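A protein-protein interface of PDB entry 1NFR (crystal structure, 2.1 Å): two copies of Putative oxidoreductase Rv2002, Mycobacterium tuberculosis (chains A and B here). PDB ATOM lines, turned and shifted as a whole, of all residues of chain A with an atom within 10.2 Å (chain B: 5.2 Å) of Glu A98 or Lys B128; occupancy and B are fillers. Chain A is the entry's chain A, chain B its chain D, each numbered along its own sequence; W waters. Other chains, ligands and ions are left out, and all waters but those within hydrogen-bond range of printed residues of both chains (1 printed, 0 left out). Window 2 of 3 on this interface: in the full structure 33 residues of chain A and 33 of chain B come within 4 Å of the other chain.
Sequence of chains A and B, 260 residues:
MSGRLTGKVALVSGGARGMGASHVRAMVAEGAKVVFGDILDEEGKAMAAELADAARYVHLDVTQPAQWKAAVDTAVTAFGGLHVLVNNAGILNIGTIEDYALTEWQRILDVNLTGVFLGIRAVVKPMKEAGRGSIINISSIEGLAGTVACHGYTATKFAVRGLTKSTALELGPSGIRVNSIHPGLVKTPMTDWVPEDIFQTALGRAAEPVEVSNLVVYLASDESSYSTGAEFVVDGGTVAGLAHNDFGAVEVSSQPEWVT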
ATOM      1  N   ILE A  94       8.070  19.033 -18.109  1.00  0.00           N
ATOM      2  CA  ILE A  94       8.304  18.908 -19.539  1.00  0.00           C
ATOM      3  C   ILE A  94       9.249  17.762 -19.853  1.00  0.00           C
ATOM      4  O   ILE A  94       9.828  17.165 -18.943  1.00  0.00           O
ATOM      5  CB  ILE A  94       8.908  20.203 -20.100  1.00  0.00           C
ATOM      6  CG1 ILE A  94      10.333  20.381 -19.581  1.00  0.00           C
ATOM      7  CG2 ILE A  94       8.074  21.389 -19.657  1.00  0.00           C
ATOM      8  CD1 ILE A  94      11.043  21.616 -20.124  1.00  0.00           C
ATOM      9  N   GLY A  95       9.411  17.471 -21.142  1.00  0.00           N
ATOM     10  CA  GLY A  95      10.301  16.400 -21.547  1.00  0.00           C
ATOM     11  C   GLY A  95       9.930  15.754 -22.871  1.00  0.00           C
ATOM     12  O   GLY A  95       8.752  15.564 -23.173  1.00  0.00           O
ATOM     13  N   THR A  96      10.943  15.410 -23.663  1.00  0.00           N
ATOM     14  CA  THR A  96      10.715  14.776 -24.950  1.00  0.00           C
ATOM     15  C   THR A  96      10.095  13.404 -24.755  1.00  0.00           C
ATOM     16  O   THR A  96      10.054  12.874 -23.644  1.00  0.00           O
ATOM     17  CB  THR A  96      12.022  14.593 -25.740  1.00  0.00           C
ATOM     18  OG1 THR A  96      12.944  13.820 -24.958  1.00  0.00           O
ATOM     19  CG2 THR A  96      12.642  15.946 -26.082  1.00  0.00           C
ATOM     20  N   ILE A  97       9.615  12.832 -25.850  1.00  0.00           N
ATOM     21  CA  ILE A  97       9.004  11.516 -25.812  1.00  0.00           C
ATOM     22  C   ILE A  97       9.986  10.487 -25.245  1.00  0.00           C
ATOM     23  O   ILE A  97       9.605   9.632 -24.451  1.00  0.00           O
ATOM     24  CB  ILE A  97       8.563  11.080 -27.232  1.00  0.00           C
ATOM     25  CG1 ILE A  97       7.422  11.985 -27.718  1.00  0.00           C
ATOM     26  CG2 ILE A  97       8.155   9.621 -27.225  1.00  0.00           C
ATOM     27  CD1 ILE A  97       6.974  11.721 -29.150  1.00  0.00           C
ATOM     28  N   GLU A  98      11.252  10.585 -25.635  1.00  0.00           N
ATOM     29  CA  GLU A  98      12.256   9.640 -25.159  1.00  0.00           C
ATOM     30  C   GLU A  98      12.710   9.799 -23.709  1.00  0.00           C
ATOM     31  O   GLU A  98      12.871   8.808 -22.998  1.00  0.00           O
ATOM     32  CB  GLU A  98      13.498   9.678 -26.056  1.00  0.00           C
ATOM     33  CG  GLU A  98      13.240   9.260 -27.494  1.00  0.00           C
ATOM     34  CD  GLU A  98      12.755  10.410 -28.352  1.00  0.00           C
ATOM     35  OE1 GLU A  98      12.379  11.468 -27.791  1.00  0.00           O
ATOM     36  OE2 GLU A  98      12.751  10.249 -29.591  1.00  0.00           O
ATOM     37  N   ASP A  99      12.905  11.032 -23.259  1.00  0.00           N
ATOM     38  CA  ASP A  99      13.408  11.256 -21.905  1.00  0.00           C
ATOM     39  C   ASP A  99      12.382  11.507 -20.797  1.00  0.00           C
ATOM     40  O   ASP A  99      12.691  11.354 -19.615  1.00  0.00           O
ATOM     41  CB  ASP A  99      14.417  12.405 -21.923  1.00  0.00           C
ATOM     42  CG  ASP A  99      13.760  13.758 -21.778  1.00  0.00           C
ATOM     43  OD1 ASP A  99      13.043  13.965 -20.772  1.00  0.00           O
ATOM     44  OD2 ASP A  99      13.962  14.620 -22.659  1.00  0.00           O
ATOM     45  N   TYR A 100      11.174  11.906 -21.164  1.00  0.00           N
ATOM     46  CA  TYR A 100      10.139  12.172 -20.170  1.00  0.00           C
ATOM     47  C   TYR A 100       9.959  10.938 -19.268  1.00  0.00           C
ATOM     48  O   TYR A 100       9.642   9.851 -19.745  1.00  0.00           O
ATOM     49  CB  TYR A 100       8.830  12.519 -20.889  1.00  0.00           C
ATOM     50  CG  TYR A 100       7.752  13.108 -20.011  1.00  0.00           C
ATOM     51  CD1 TYR A 100       7.973  14.275 -19.279  1.00  0.00           C
ATOM     52  CD2 TYR A 100       6.496  12.517 -19.943  1.00  0.00           C
ATOM     53  CE1 TYR A 100       6.962  14.840 -18.503  1.00  0.00           C
ATOM     54  CE2 TYR A 100       5.480  13.068 -19.172  1.00  0.00           C
ATOM     55  CZ  TYR A 100       5.714  14.228 -18.456  1.00  0.00           C
ATOM     56  OH  TYR A 100       4.694  14.773 -17.711  1.00  0.00           O
ATOM     57  N   ALA A 101      10.174  11.108 -17.967  1.00  0.00           N
ATOM     58  CA  ALA A 101      10.032   9.999 -17.024  1.00  0.00           C
ATOM     59  C   ALA A 101       8.570   9.585 -16.879  1.00  0.00           C
ATOM     60  O   ALA A 101       7.687  10.436 -16.777  1.00  0.00           O
ATOM     61  CB  ALA A 101      10.600  10.398 -15.667  1.00  0.00           C
ATOM     62  N   LEU A 102       8.314   8.280 -16.867  1.00  0.00           N
ATOM     63  CA  LEU A 102       6.951   7.776 -16.724  1.00  0.00           C
ATOM     64  C   LEU A 102       6.356   8.138 -15.368  1.00  0.00           C
ATOM     65  O   LEU A 102       5.133   8.184 -15.212  1.00  0.00           O
ATOM     66  CB  LEU A 102       6.910   6.259 -16.924  1.00  0.00           C
ATOM     67  CG  LEU A 102       7.091   5.777 -18.368  1.00  0.00           C
ATOM     68  CD1 LEU A 102       6.895   4.271 -18.427  1.00  0.00           C
ATOM     69  CD2 LEU A 102       6.093   6.476 -19.281  1.00  0.00           C
ATOM     70  N   GLU A 104       6.831  11.055 -13.970  1.00  0.00           N
ATOM     71  CA  GLU A 104       6.412  12.455 -14.119  1.00  0.00           C
ATOM     72  C   GLU A 104       5.043  12.449 -14.792  1.00  0.00           C
ATOM     73  O   GLU A 104       4.148  13.216 -14.427  1.00  0.00           O
ATOM     74  CB  GLU A 104       7.362  13.245 -15.031  1.00  0.00           C
ATOM     75  CG  GLU A 104       8.826  13.303 -14.635  1.00  0.00           C
ATOM     76  CD  GLU A 104       9.658  14.038 -15.690  1.00  0.00           C
ATOM     77  OE1 GLU A 104       9.474  15.273 -15.838  1.00  0.00           O
ATOM     78  OE2 GLU A 104      10.480  13.383 -16.382  1.00  0.00           O
ATOM     79  N   VAL A 148       5.725  21.141 -28.000  1.00  0.00           N
ATOM     80  CA  VAL A 148       6.818  20.164 -27.999  1.00  0.00           C
ATOM     81  C   VAL A 148       7.323  19.880 -26.577  1.00  0.00           C
ATOM     82  O   VAL A 148       7.370  20.778 -25.736  1.00  0.00           O
ATOM     83  CB  VAL A 148       8.001  20.659 -28.884  1.00  0.00           C
ATOM     84  CG1 VAL A 148       9.179  19.672 -28.819  1.00  0.00           C
ATOM     85  CG2 VAL A 148       7.530  20.813 -30.320  1.00  0.00           C
ATOM     86  N   ALA A 149       7.677  18.622 -26.316  1.00  0.00           N
ATOM     87  CA  ALA A 149       8.182  18.196 -25.007  1.00  0.00           C
ATOM     88  C   ALA A 149       7.260  18.613 -23.867  1.00  0.00           C
ATOM     89  O   ALA A 149       7.712  18.876 -22.754  1.00  0.00           O
ATOM     90  CB  ALA A 149       9.587  18.767 -24.779  1.00  0.00           C
ATOM     91  N   CYS A 150       5.961  18.643 -24.139  1.00  0.00           N
ATOM     92  CA  CYS A 150       4.978  19.067 -23.139  1.00  0.00           C
ATOM     93  C   CYS A 150       3.783  18.114 -23.171  1.00  0.00           C
ATOM     94  O   CYS A 150       2.629  18.532 -23.053  1.00  0.00           O
ATOM     95  CB  CYS A 150       4.534  20.488 -23.484  1.00  0.00           C
ATOM     96  SG  CYS A 150       3.715  21.402 -22.188  1.00  0.00           S
ATOM     97  N   HIS A 151       4.080  16.830 -23.312  1.00  0.00           N
ATOM     98  CA  HIS A 151       3.070  15.782 -23.423  1.00  0.00           C
ATOM     99  C   HIS A 151       2.167  15.563 -22.214  1.00  0.00           C
ATOM    100  O   HIS A 151       0.947  15.448 -22.356  1.00  0.00           O
ATOM    101  CB  HIS A 151       3.781  14.489 -23.823  1.00  0.00           C
ATOM    102  CG  HIS A 151       4.737  14.682 -24.955  1.00  0.00           C
ATOM    103  ND1 HIS A 151       4.327  15.108 -26.201  1.00  0.00           N
ATOM    104  CD2 HIS A 151       6.089  14.626 -25.001  1.00  0.00           C
ATOM    105  CE1 HIS A 151       5.387  15.315 -26.963  1.00  0.00           C
ATOM    106  NE2 HIS A 151       6.469  15.031 -26.259  1.00  0.00           N
ATOM    107  N   ARG B 121       6.061   6.002 -27.471  1.00  0.00           N
ATOM    108  CA  ARG B 121       7.434   5.911 -26.961  1.00  0.00           C
ATOM    109  C   ARG B 121       8.159   4.726 -27.584  1.00  0.00           C
ATOM    110  O   ARG B 121       9.325   4.826 -27.970  1.00  0.00           O
ATOM    111  CB  ARG B 121       7.428   5.740 -25.437  1.00  0.00           C
ATOM    112  CG  ARG B 121       6.716   6.853 -24.691  1.00  0.00           C
ATOM    113  CD  ARG B 121       6.420   6.478 -23.243  1.00  0.00           C
ATOM    114  NE  ARG B 121       7.541   6.714 -22.336  1.00  0.00           N
ATOM    115  CZ  ARG B 121       8.446   5.805 -21.992  1.00  0.00           C
ATOM    116  NH1 ARG B 121       8.383   4.563 -22.478  1.00  0.00           N
ATOM    117  NH2 ARG B 121       9.405   6.133 -21.136  1.00  0.00           N
ATOM    118  N   VAL B 123       7.585   3.165 -30.521  1.00  0.00           N
ATOM    119  CA  VAL B 123       7.821   3.151 -31.964  1.00  0.00           C
ATOM    120  C   VAL B 123       8.684   4.252 -32.568  1.00  0.00           C
ATOM    121  O   VAL B 123       9.103   4.132 -33.721  1.00  0.00           O
ATOM    122  CB  VAL B 123       6.486   3.133 -32.757  1.00  0.00           C
ATOM    123  CG1 VAL B 123       5.603   2.001 -32.271  1.00  0.00           C
ATOM    124  CG2 VAL B 123       5.779   4.468 -32.624  1.00  0.00           C
ATOM    125  N   VAL B 124       8.965   5.310 -31.812  1.00  0.00           N
ATOM    126  CA  VAL B 124       9.754   6.420 -32.354  1.00  0.00           C
ATOM    127  C   VAL B 124      11.184   6.109 -32.800  1.00  0.00           C
ATOM    128  O   VAL B 124      11.653   6.668 -33.792  1.00  0.00           O
ATOM    129  CB  VAL B 124       9.804   7.619 -31.376  1.00  0.00           C
ATOM    130  CG1 VAL B 124       8.446   8.304 -31.314  1.00  0.00           C
ATOM    131  CG2 VAL B 124      10.226   7.150 -29.996  1.00  0.00           C
ATOM    132  N   LYS B 125      11.882   5.227 -32.091  1.00  0.00           N
ATOM    133  CA  LYS B 125      13.258   4.921 -32.483  1.00  0.00           C
ATOM    134  C   LYS B 125      13.343   4.314 -33.878  1.00  0.00           C
ATOM    135  O   LYS B 125      14.075   4.812 -34.724  1.00  0.00           O
ATOM    136  CB  LYS B 125      13.942   3.999 -31.467  1.00  0.00           C
ATOM    137  CG  LYS B 125      15.425   3.792 -31.780  1.00  0.00           C
ATOM    138  CD  LYS B 125      16.169   3.024 -30.692  1.00  0.00           C
ATOM    139  CE  LYS B 125      17.647   2.871 -31.057  1.00  0.00           C
ATOM    140  NZ  LYS B 125      18.444   2.246 -29.963  1.00  0.00           N
ATOM    141  N   PRO B 126      12.600   3.228 -34.142  1.00  0.00           N
ATOM    142  CA  PRO B 126      12.674   2.643 -35.484  1.00  0.00           C
ATOM    143  C   PRO B 126      12.113   3.565 -36.578  1.00  0.00           C
ATOM    144  O   PRO B 126      12.479   3.449 -37.752  1.00  0.00           O
ATOM    145  CB  PRO B 126      11.885   1.343 -35.337  1.00  0.00           C
ATOM    146  CG  PRO B 126      10.888   1.668 -34.278  1.00  0.00           C
ATOM    147  CD  PRO B 126      11.715   2.436 -33.273  1.00  0.00           C
ATOM    148  N   MET B 127      11.227   4.483 -36.200  1.00  0.00           N
ATOM    149  CA  MET B 127      10.664   5.404 -37.181  1.00  0.00           C
ATOM    150  C   MET B 127      11.653   6.529 -37.445  1.00  0.00           C
ATOM    151  O   MET B 127      11.784   6.999 -38.577  1.00  0.00           O
ATOM    152  CB  MET B 127       9.341   5.998 -36.692  1.00  0.00           C
ATOM    153  CG  MET B 127       8.222   4.982 -36.450  1.00  0.00           C
ATOM    154  SD  MET B 127       6.488   5.844 -36.254  1.00  0.00           S
ATOM    155  CE  MET B 127       6.903   7.021 -34.801  1.00  0.00           C
ATOM    156  N   LYS B 128      12.354   6.958 -36.399  1.00  0.00           N
ATOM    157  CA  LYS B 128      13.331   8.030 -36.541  1.00  0.00           C
ATOM    158  C   LYS B 128      14.569   7.610 -37.345  1.00  0.00           C
ATOM    159  O   LYS B 128      15.304   8.461 -37.856  1.00  0.00           O
ATOM    160  CB  LYS B 128      13.759   8.551 -35.167  1.00  0.00           C
ATOM    161  CG  LYS B 128      12.706   9.407 -34.476  1.00  0.00           C
ATOM    162  CD  LYS B 128      13.307  10.204 -33.326  1.00  0.00           C
ATOM    163  CE  LYS B 128      12.286  11.172 -32.739  1.00  0.00           C
ATOM    164  NZ  LYS B 128      12.845  11.999 -31.629  1.00  0.00           N
ATOM    165  N   GLU B 129      14.800   6.304 -37.455  1.00  0.00           N
ATOM    166  CA  GLU B 129      15.952   5.813 -38.202  1.00  0.00           C
ATOM    167  C   GLU B 129      15.645   5.860 -39.690  1.00  0.00           C
ATOM    168  O   GLU B 129      16.516   6.168 -40.503  1.00  0.00           O
ATOM    169  CB  GLU B 129      16.294   4.384 -37.779  1.00  0.00           C
ATOM    170  CG  GLU B 129      16.547   4.235 -36.284  1.00  0.00           C
ATOM    171  CD  GLU B 129      17.031   2.852 -35.903  1.00  0.00           C
ATOM    172  OE1 GLU B 129      16.586   1.864 -36.524  1.00  0.00           O
ATOM    173  OE2 GLU B 129      17.850   2.750 -34.965  1.00  0.00           O
ATOM    174  N   ALA B 130      14.397   5.561 -40.036  1.00  0.00           N
ATOM    175  CA  ALA B 130      13.955   5.573 -41.425  1.00  0.00           C
ATOM    176  C   ALA B 130      13.461   6.964 -41.807  1.00  0.00           C
ATOM    177  O   ALA B 130      13.091   7.199 -42.955  1.00  0.00           O
ATOM    178  CB  ALA B 130      12.841   4.545 -41.631  1.00  0.00           C
ATOM    179  N   GLY B 131      13.457   7.877 -40.836  1.00  0.00           N
ATOM    180  CA  GLY B 131      13.011   9.240 -41.080  1.00  0.00           C
ATOM    181  C   GLY B 131      11.631   9.304 -41.710  1.00  0.00           C
ATOM    182  O   GLY B 131      11.332  10.199 -42.500  1.00  0.00           O
ATOM    183  N   GLU B 170       6.534  17.564 -32.093  1.00  0.00           N
ATOM    184  CA  GLU B 170       7.863  17.098 -31.724  1.00  0.00           C
ATOM    185  C   GLU B 170       8.467  16.105 -32.712  1.00  0.00           C
ATOM    186  O   GLU B 170       9.677  16.098 -32.918  1.00  0.00           O
ATOM    187  CB  GLU B 170       7.816  16.469 -30.321  1.00  0.00           C
ATOM    188  CG  GLU B 170       9.167  16.031 -29.768  1.00  0.00           C
ATOM    189  CD  GLU B 170       9.072  15.510 -28.344  1.00  0.00           C
ATOM    190  OE1 GLU B 170       8.486  16.209 -27.485  1.00  0.00           O
ATOM    191  OE2 GLU B 170       9.588  14.404 -28.078  1.00  0.00           O
ATOM    192  N   LEU B 171       7.628  15.280 -33.333  1.00  0.00           N
ATOM    193  CA  LEU B 171       8.117  14.267 -34.263  1.00  0.00           C
ATOM    194  C   LEU B 171       8.189  14.709 -35.723  1.00  0.00           C
ATOM    195  O   LEU B 171       8.833  14.052 -36.540  1.00  0.00           O
ATOM    196  CB  LEU B 171       7.257  13.000 -34.146  1.00  0.00           C
ATOM    197  CG  LEU B 171       7.231  12.304 -32.778  1.00  0.00           C
ATOM    198  CD1 LEU B 171       6.303  11.095 -32.823  1.00  0.00           C
ATOM    199  CD2 LEU B 171       8.638  11.881 -32.390  1.00  0.00           C
ATOM    200  N   SER B 174      11.386  14.806 -37.614  1.00  0.00           N
ATOM    201  CA  SER B 174      11.922  13.478 -37.918  1.00  0.00           C
ATOM    202  C   SER B 174      11.160  12.809 -39.051  1.00  0.00           C
ATOM    203  O   SER B 174      11.463  11.678 -39.430  1.00  0.00           O
ATOM    204  CB  SER B 174      11.877  12.589 -36.679  1.00  0.00           C
ATOM    205  OG  SER B 174      12.708  13.102 -35.659  1.00  0.00           O
ATOM    206  N   ILE B 176       7.924  12.125 -38.968  1.00  0.00           N
ATOM    207  CA  ILE B 176       6.880  11.269 -38.426  1.00  0.00           C
ATOM    208  C   ILE B 176       5.608  12.051 -38.192  1.00  0.00           C
ATOM    209  O   ILE B 176       5.596  13.003 -37.410  1.00  0.00           O
ATOM    210  CB  ILE B 176       7.276  10.665 -37.088  1.00  0.00           C
ATOM    211  CG1 ILE B 176       8.602   9.918 -37.223  1.00  0.00           C
ATOM    212  CG2 ILE B 176       6.161   9.735 -36.608  1.00  0.00           C
ATOM    213  CD1 ILE B 176       9.176   9.472 -35.903  1.00  0.00           C
HETATM  214  O   HOH W   1      11.395  13.297 -29.832  1.00  0.00           O
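The backbone NH (N) of Ala A149 is in hydrogen-bond range of the side-chain carboxylate (OE1) of Glu B170 (2.8 Å).
A ring nitrogen (NE2) of His A151 sits at hydrogen-bond distance from the side-chain carboxylate (OE1) of Glu B170.
The side-chain carboxylate of Glu A98 is in salt-bridge range of the side-chain amino group of Lys B128, at 2.7 Å.
The backbone NH (N) of Ile A97 is in hydrogen-bond range of the side-chain carboxylate (OE2) of Glu B170 (2.7 Å).
OG1 of Thr A96 sits at hydrogen-bond distance from OD2 of Asp A99, at 2.6 Å.
The backbone NH (N) of Ile B176 sits at hydrogen-bond distance from the backbone carbonyl oxygen (O) of Leu B171, 3.2 Å away.
N of Gly A95 sits at hydrogen-bond distance from O of Ala A149 (2.7 Å).
Among the printed residues, pairs that only touch across the chains: Thr A96 with Glu B170 (3.3 Å), Ile A97 with Arg B121 (3.8 Å), Ile A97 with Leu B171 (3.6 Å), Tyr A100 with Arg B121 (3.98 Å), Leu A102 with Arg B121 (3.4 Å) and Val A148 with Glu B170 (3.8 Å).
Of chain A, only Glu A98 (2.7 Å) comes within 4 Å of Lys B128.
No residue of chain A comes within 4 Å of Pro B126.
No residue of chain A comes within 4 Å of Ala B130.
Ser B174 touches none of the printed residues of chain A.
Printed residues of chain B within 4 Å of Val A148: Glu B170.
Of the printed residues of chain B, Thr A96 touches Glu B170 (3.3 Å).
Of the printed residues of chain B, Leu A102 touches Arg B121 (3.4 Å).
The nearest printed residue of chain B that does not touch Glu A98 is Val B124 (4.02 Å).
The nearest residue of chain A that does not touch Lys B128 is Ile A97 (6.2 Å).
The nearest printed residue of chain B that does not touch His A151 is Leu B171 (6.8 Å).
Of the 14 printed residues of chain B, 4 touch a printed residue of chain A.
Printed residues of chain B that touch a printed residue of chain A: Arg B121, Lys B128, Glu B170 and Leu B171.
Along chain B the printed residues that touch a printed residue of chain A span positions 121 to 171.
Hydrophobic or aromatic side chains of chain A that line the printed part of chain B: Ile A97, Leu A102, Val A148, Ala A149 and His A151.
Among the printed residues, Asp or Glu carboxylates within 4 Å of a Lys or Arg side-chain nitrogen of the other chain: Glu A98 with Lys B128 (2.7 Å).
No position is printed for both chains.
Of the 10 pairs that touch across the chains among the printed residues, none has its exchanged pair printed and touching as well.
Water W1 lies within hydrogen-bond range of the side-chain amino group of Lys B128 (2.6 Å), the side-chain carboxylate of Glu B170 (2.8 Å) and the side-chain carboxylate of Glu A98 (2.9 Å).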
